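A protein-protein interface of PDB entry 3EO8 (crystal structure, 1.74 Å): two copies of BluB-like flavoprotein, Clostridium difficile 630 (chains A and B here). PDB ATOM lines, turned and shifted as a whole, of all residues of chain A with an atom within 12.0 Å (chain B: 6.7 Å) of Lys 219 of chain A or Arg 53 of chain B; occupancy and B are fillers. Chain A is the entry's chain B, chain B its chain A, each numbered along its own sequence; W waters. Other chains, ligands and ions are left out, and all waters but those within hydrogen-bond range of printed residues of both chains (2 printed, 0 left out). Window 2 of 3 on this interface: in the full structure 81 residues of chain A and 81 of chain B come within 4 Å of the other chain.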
ATOM      1  N   CYS A 215      10.464   0.445 -32.449  1.00  0.00           N
ATOM      2  CA  CYS A 215      10.377  -0.747 -31.648  1.00  0.00           C
ATOM      3  C   CYS A 215      11.713  -1.382 -31.356  1.00  0.00           C
ATOM      4  O   CYS A 215      12.691  -1.180 -32.078  1.00  0.00           O
ATOM      5  CB  CYS A 215       9.426  -1.761 -32.272  1.00  0.00           C
ATOM      6  SG  CYS A 215       9.900  -2.518 -33.867  1.00  0.00           S
ATOM      7  N   THR A 216      11.705  -2.180 -30.298  1.00  0.00           N
ATOM      8  CA  THR A 216      12.853  -2.985 -29.915  1.00  0.00           C
ATOM      9  C   THR A 216      12.345  -4.369 -29.498  1.00  0.00           C
ATOM     10  O   THR A 216      11.529  -4.477 -28.600  1.00  0.00           O
ATOM     11  CB  THR A 216      13.594  -2.319 -28.768  1.00  0.00           C
ATOM     12  OG1 THR A 216      14.060  -1.041 -29.207  1.00  0.00           O
ATOM     13  CG2 THR A 216      14.778  -3.179 -28.312  1.00  0.00           C
ATOM     14  N   PHE A 217      12.823  -5.419 -30.165  1.00  0.00           N
ATOM     15  CA  PHE A 217      12.505  -6.781 -29.768  1.00  0.00           C
ATOM     16  C   PHE A 217      13.582  -7.308 -28.819  1.00  0.00           C
ATOM     17  O   PHE A 217      14.725  -7.523 -29.223  1.00  0.00           O
ATOM     18  CB  PHE A 217      12.381  -7.694 -31.004  1.00  0.00           C
ATOM     19  CG  PHE A 217      11.084  -7.530 -31.770  1.00  0.00           C
ATOM     20  CD1 PHE A 217      10.817  -6.373 -32.459  1.00  0.00           C
ATOM     21  CD2 PHE A 217      10.140  -8.548 -31.801  1.00  0.00           C
ATOM     22  CE1 PHE A 217       9.643  -6.228 -33.159  1.00  0.00           C
ATOM     23  CE2 PHE A 217       8.947  -8.393 -32.519  1.00  0.00           C
ATOM     24  CZ  PHE A 217       8.702  -7.234 -33.176  1.00  0.00           C
ATOM     25  N   ILE A 218      13.238  -7.512 -27.555  1.00  0.00           N
ATOM     26  CA  ILE A 218      14.216  -8.028 -26.594  1.00  0.00           C
ATOM     27  C   ILE A 218      14.533  -9.475 -26.928  1.00  0.00           C
ATOM     28  O   ILE A 218      13.629 -10.281 -27.119  1.00  0.00           O
ATOM     29  CB  ILE A 218      13.698  -7.910 -25.155  1.00  0.00           C
ATOM     30  CG1 ILE A 218      13.476  -6.447 -24.799  1.00  0.00           C
ATOM     31  CG2 ILE A 218      14.680  -8.548 -24.109  1.00  0.00           C
ATOM     32  CD1 ILE A 218      14.557  -5.508 -25.261  1.00  0.00           C
ATOM     33  N   LYS A 219      15.823  -9.800 -26.989  1.00  0.00           N
ATOM     34  CA  LYS A 219      16.253 -11.145 -27.351  1.00  0.00           C
ATOM     35  C   LYS A 219      16.670 -11.863 -26.074  1.00  0.00           C
ATOM     36  O   LYS A 219      17.394 -11.266 -25.281  1.00  0.00           O
ATOM     37  CB  LYS A 219      17.399 -11.087 -28.375  1.00  0.00           C
ATOM     38  OXT LYS A 219      16.299 -13.016 -25.781  1.00  0.00           O
ATOM     39  N   VAL B  50       9.167  -5.191 -27.218  1.00  0.00           N
ATOM     40  CA  VAL B  50       8.498  -6.476 -27.261  1.00  0.00           C
ATOM     41  C   VAL B  50       9.259  -7.548 -26.479  1.00  0.00           C
ATOM     42  O   VAL B  50      10.422  -7.849 -26.784  1.00  0.00           O
ATOM     43  CB  VAL B  50       8.378  -6.933 -28.713  1.00  0.00           C
ATOM     44  CG1 VAL B  50       7.669  -8.283 -28.767  1.00  0.00           C
ATOM     45  CG2 VAL B  50       7.598  -5.902 -29.519  1.00  0.00           C
ATOM     46  N   ILE B  51       8.613  -8.128 -25.470  1.00  0.00           N
ATOM     47  CA  ILE B  51       9.266  -9.083 -24.600  1.00  0.00           C
ATOM     48  C   ILE B  51       8.582 -10.421 -24.636  1.00  0.00           C
ATOM     49  O   ILE B  51       7.380 -10.509 -24.434  1.00  0.00           O
ATOM     50  CB  ILE B  51       9.265  -8.580 -23.135  1.00  0.00           C
ATOM     51  CG1 ILE B  51      10.024  -7.281 -23.027  1.00  0.00           C
ATOM     52  CG2 ILE B  51       9.915  -9.606 -22.194  1.00  0.00           C
ATOM     53  CD1 ILE B  51       9.701  -6.501 -21.759  1.00  0.00           C
ATOM     54  N   LYS B  52       9.375 -11.469 -24.888  1.00  0.00           N
ATOM     55  CA  LYS B  52       8.947 -12.849 -24.735  1.00  0.00           C
ATOM     56  C   LYS B  52       9.754 -13.581 -23.656  1.00  0.00           C
ATOM     57  O   LYS B  52       9.411 -14.715 -23.287  1.00  0.00           O
ATOM     58  CB  LYS B  52       9.059 -13.590 -26.078  1.00  0.00           C
ATOM     59  CG  LYS B  52       8.004 -13.195 -27.112  1.00  0.00           C
ATOM     60  CD  LYS B  52       8.282 -13.862 -28.461  1.00  0.00           C
ATOM     61  CE  LYS B  52       7.340 -13.415 -29.554  1.00  0.00           C
ATOM     62  NZ  LYS B  52       7.630 -14.204 -30.786  1.00  0.00           N
ATOM     63  N   ARG B  53      10.788 -12.931 -23.132  1.00  0.00           N
ATOM     64  CA  ARG B  53      11.678 -13.587 -22.171  1.00  0.00           C
ATOM     65  C   ARG B  53      10.963 -13.727 -20.829  1.00  0.00           C
ATOM     66  O   ARG B  53      10.641 -12.748 -20.180  1.00  0.00           O
ATOM     67  CB  ARG B  53      12.989 -12.798 -22.023  1.00  0.00           C
ATOM     68  CG  ARG B  53      14.114 -13.598 -21.399  1.00  0.00           C
ATOM     69  CD  ARG B  53      15.230 -12.705 -20.863  1.00  0.00           C
ATOM     70  NE  ARG B  53      15.945 -11.993 -21.917  1.00  0.00           N
ATOM     71  CZ  ARG B  53      16.599 -10.844 -21.761  1.00  0.00           C
ATOM     72  NH1 ARG B  53      16.610 -10.208 -20.593  1.00  0.00           N
ATOM     73  NH2 ARG B  53      17.223 -10.306 -22.791  1.00  0.00           N
ATOM     74  N   ARG B  54      10.706 -14.972 -20.416  1.00  0.00           N
ATOM     75  CA  ARG B  54       9.875 -15.219 -19.216  1.00  0.00           C
ATOM     76  C   ARG B  54      10.474 -14.596 -17.981  1.00  0.00           C
ATOM     77  O   ARG B  54       9.751 -14.008 -17.175  1.00  0.00           O
ATOM     78  CB  ARG B  54       9.658 -16.699 -18.901  1.00  0.00           C
ATOM     79  CG  ARG B  54       8.895 -17.506 -19.910  1.00  0.00           C
ATOM     80  CD  ARG B  54       7.498 -16.956 -20.192  1.00  0.00           C
ATOM     81  NE  ARG B  54       6.732 -16.520 -19.032  1.00  0.00           N
ATOM     82  CZ  ARG B  54       5.479 -16.059 -19.120  1.00  0.00           C
ATOM     83  NH1 ARG B  54       4.857 -16.015 -20.302  1.00  0.00           N
ATOM     84  NH2 ARG B  54       4.846 -15.628 -18.019  1.00  0.00           N
ATOM     85  N   ASP B  55      11.790 -14.703 -17.819  1.00  0.00           N
ATOM     86  CA  ASP B  55      12.367 -14.242 -16.569  1.00  0.00           C
ATOM     87  C   ASP B  55      12.260 -12.737 -16.429  1.00  0.00           C
ATOM     88  O   ASP B  55      12.196 -12.242 -15.317  1.00  0.00           O
ATOM     89  CB  ASP B  55      13.812 -14.689 -16.392  1.00  0.00           C
ATOM     90  CG  ASP B  55      14.757 -13.875 -17.212  1.00  0.00           C
ATOM     91  OD1 ASP B  55      14.814 -14.129 -18.433  1.00  0.00           O
ATOM     92  OD2 ASP B  55      15.404 -12.957 -16.636  1.00  0.00           O
ATOM     93  N   LEU B  56      12.316 -12.004 -17.542  1.00  0.00           N
ATOM     94  CA  LEU B  56      12.140 -10.550 -17.498  1.00  0.00           C
ATOM     95  C   LEU B  56      10.692 -10.199 -17.138  1.00  0.00           C
ATOM     96  O   LEU B  56      10.428  -9.310 -16.341  1.00  0.00           O
ATOM     97  CB  LEU B  56      12.555  -9.941 -18.845  1.00  0.00           C
ATOM     98  CG  LEU B  56      12.423  -8.448 -19.056  1.00  0.00           C
ATOM     99  CD1 LEU B  56      13.058  -7.645 -17.919  1.00  0.00           C
ATOM    100  CD2 LEU B  56      13.063  -8.103 -20.399  1.00  0.00           C
ATOM    101  N   MET B  57       9.741 -10.921 -17.719  1.00  0.00           N
ATOM    102  CA  MET B  57       8.319 -10.741 -17.360  1.00  0.00           C
ATOM    103  C   MET B  57       8.110 -10.971 -15.866  1.00  0.00           C
ATOM    104  O   MET B  57       7.344 -10.254 -15.217  1.00  0.00           O
ATOM    105  CB  MET B  57       7.433 -11.703 -18.185  1.00  0.00           C
ATOM    106  CG  MET B  57       7.343 -11.297 -19.630  1.00  0.00           C
ATOM    107  SD  MET B  57       6.582 -12.666 -20.798  1.00  0.00           S
ATOM    108  CE  MET B  57       4.765 -12.416 -20.248  1.00  0.00           C
ATOM    109  N   GLU B  58       8.810 -11.943 -15.295  1.00  0.00           N
ATOM    110  CA  GLU B  58       8.638 -12.230 -13.873  1.00  0.00           C
ATOM    111  C   GLU B  58       9.324 -11.164 -13.041  1.00  0.00           C
ATOM    112  O   GLU B  58       8.847 -10.793 -11.960  1.00  0.00           O
ATOM    113  CB  GLU B  58       9.233 -13.590 -13.512  1.00  0.00           C
ATOM    114  CG  GLU B  58       8.541 -14.755 -14.212  1.00  0.00           C
ATOM    115  CD  GLU B  58       7.200 -15.118 -13.602  1.00  0.00           C
ATOM    116  OE1 GLU B  58       6.865 -14.563 -12.520  1.00  0.00           O
ATOM    117  OE2 GLU B  58       6.486 -15.966 -14.204  1.00  0.00           O
ATOM    118  N   PRO B 101       1.942 -15.077 -23.634  1.00  0.00           N
ATOM    119  CA  PRO B 101       3.275 -15.303 -24.166  1.00  0.00           C
ATOM    120  C   PRO B 101       4.083 -14.046 -24.460  1.00  0.00           C
ATOM    121  O   PRO B 101       5.290 -14.125 -24.551  1.00  0.00           O
ATOM    122  CB  PRO B 101       3.006 -16.100 -25.454  1.00  0.00           C
ATOM    123  CG  PRO B 101       1.624 -15.656 -25.892  1.00  0.00           C
ATOM    124  CD  PRO B 101       0.880 -15.376 -24.614  1.00  0.00           C
ATOM    125  N   LEU B 177      14.034  -3.184 -16.786  1.00  0.00           N
ATOM    126  CA  LEU B 177      14.241  -3.371 -18.219  1.00  0.00           C
ATOM    127  C   LEU B 177      15.648  -2.967 -18.607  1.00  0.00           C
ATOM    128  O   LEU B 177      16.328  -3.682 -19.353  1.00  0.00           O
ATOM    129  CB  LEU B 177      13.238  -2.524 -19.010  1.00  0.00           C
ATOM    130  CG  LEU B 177      13.337  -2.606 -20.518  1.00  0.00           C
ATOM    131  CD1 LEU B 177      13.042  -4.046 -20.999  1.00  0.00           C
ATOM    132  CD2 LEU B 177      12.379  -1.597 -21.152  1.00  0.00           C
ATOM    133  N   GLU B 180      18.440  -5.358 -17.265  1.00  0.00           N
ATOM    134  CA  GLU B 180      18.392  -6.709 -17.816  1.00  0.00           C
ATOM    135  C   GLU B 180      18.586  -6.811 -19.340  1.00  0.00           C
ATOM    136  O   GLU B 180      18.810  -7.911 -19.854  1.00  0.00           O
ATOM    137  CB  GLU B 180      17.042  -7.361 -17.481  1.00  0.00           C
ATOM    138  CG  GLU B 180      16.771  -7.563 -16.021  1.00  0.00           C
ATOM    139  CD  GLU B 180      17.712  -8.558 -15.357  1.00  0.00           C
ATOM    140  OE1 GLU B 180      18.121  -9.555 -15.980  1.00  0.00           O
ATOM    141  OE2 GLU B 180      18.025  -8.326 -14.179  1.00  0.00           O
ATOM    142  N   THR B 181      18.485  -5.698 -20.056  1.00  0.00           N
ATOM    143  CA  THR B 181      18.517  -5.718 -21.511  1.00  0.00           C
ATOM    144  C   THR B 181      19.432  -4.675 -22.165  1.00  0.00           C
ATOM    145  O   THR B 181      19.683  -4.757 -23.358  1.00  0.00           O
ATOM    146  CB  THR B 181      17.102  -5.460 -22.100  1.00  0.00           C
ATOM    147  OG1 THR B 181      16.716  -4.100 -21.880  1.00  0.00           O
ATOM    148  CG2 THR B 181      16.040  -6.401 -21.510  1.00  0.00           C
HETATM  149  O   HOH W   1      12.164 -11.546 -25.330  1.00  0.00           O
HETATM  150  O   HOH W   2      11.240  -9.859 -28.553  1.00  0.00           O
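The guanidinium group (NH2) of Arg 53 of chain B is in salt-bridge range of the chain-end carboxylate (O) of Lys 219 of chain A (2.7 Å).
The backbone NH (N) of Val 50 of chain B sits at hydrogen-bond distance from the backbone carbonyl oxygen (O) of Thr 216 of chain A (2.8 Å).
O of Val 50 of chain B is in hydrogen-bond range of N of Ile 218 of chain A, at 2.9 Å.
O of Leu 177 of chain B is in hydrogen-bond range of OG1 of Thr 181 of chain B (2.6 Å).
The guanidinium group (NH1) of Arg 53 of chain B is in hydrogen-bond range of the backbone carbonyl oxygen (O) of Glu 180 of chain B (3.3 Å).
Among the printed residues, merely in contact across the chains: Ile 218 of chain A with Arg 53 of chain B, Ile 218 of chain A with Thr 181 of chain B, Phe 217 of chain A with Val 50 of chain B and Ile 218 of chain A with Ile 51 of chain B.
Printed residues of chain B within 4 Å of Lys 219 of chain A: Arg 53 (2.7 Å).
Of the printed residues of chain A, Arg 53 of chain B touches Ile 218 (3.4 Å) and Lys 219 (2.7 Å).
Of chain A, only Ile 218 comes within 4 Å of Ile 51 of chain B.
No residue of chain A comes within 4 Å of Asp 55 of chain B.
No residue of chain A comes within 4 Å of Leu 56 of chain B.
No residue of chain A comes within 4 Å of Met 57 of chain B.
Of the printed residues of chain A, Thr 181 of chain B touches Ile 218.
Printed residues of chain B within 4 Å of Phe 217 of chain A: Val 50 (3.8 Å).
Of the printed residues of chain B, Ile 218 of chain A touches Val 50, Ile 51, Arg 53 and Thr 181.
Of the printed residues of chain B, Thr 216 of chain A touches Val 50.
Of the printed residues of chain A, Val 50 of chain B touches Thr 216, Phe 217 and Ile 218.
Pro 101 of chain B touches none of the printed residues of chain A.
The nearest printed residue of chain B that does not touch Ile 218 of chain A is Leu 56 of chain B (4.1 Å).
Of the 5 printed residues of chain A, 4 touch a printed residue of chain B.
Printed residues of chain A that touch a printed residue of chain B: Thr 216, Phe 217, Ile 218 and Lys 219.
Hydrophobic or aromatic side chains of chain A within 4 Å of the printed part of chain B: Phe 217 and Ile 218.
Along chain B the printed residues that touch a printed residue of chain A span positions 50 to 181.
No position is printed for both chains.
Water W1 lies within hydrogen-bond range of the backbone carbonyl oxygen of Ile 218 of chain A, the backbone NH of Lys 52 of chain B and the backbone NH of Arg 53 of chain B.
Water W2 bridges O of Val 50 of chain B (2.8 Å) and O of Ile 218 of chain A (2.8 Å).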
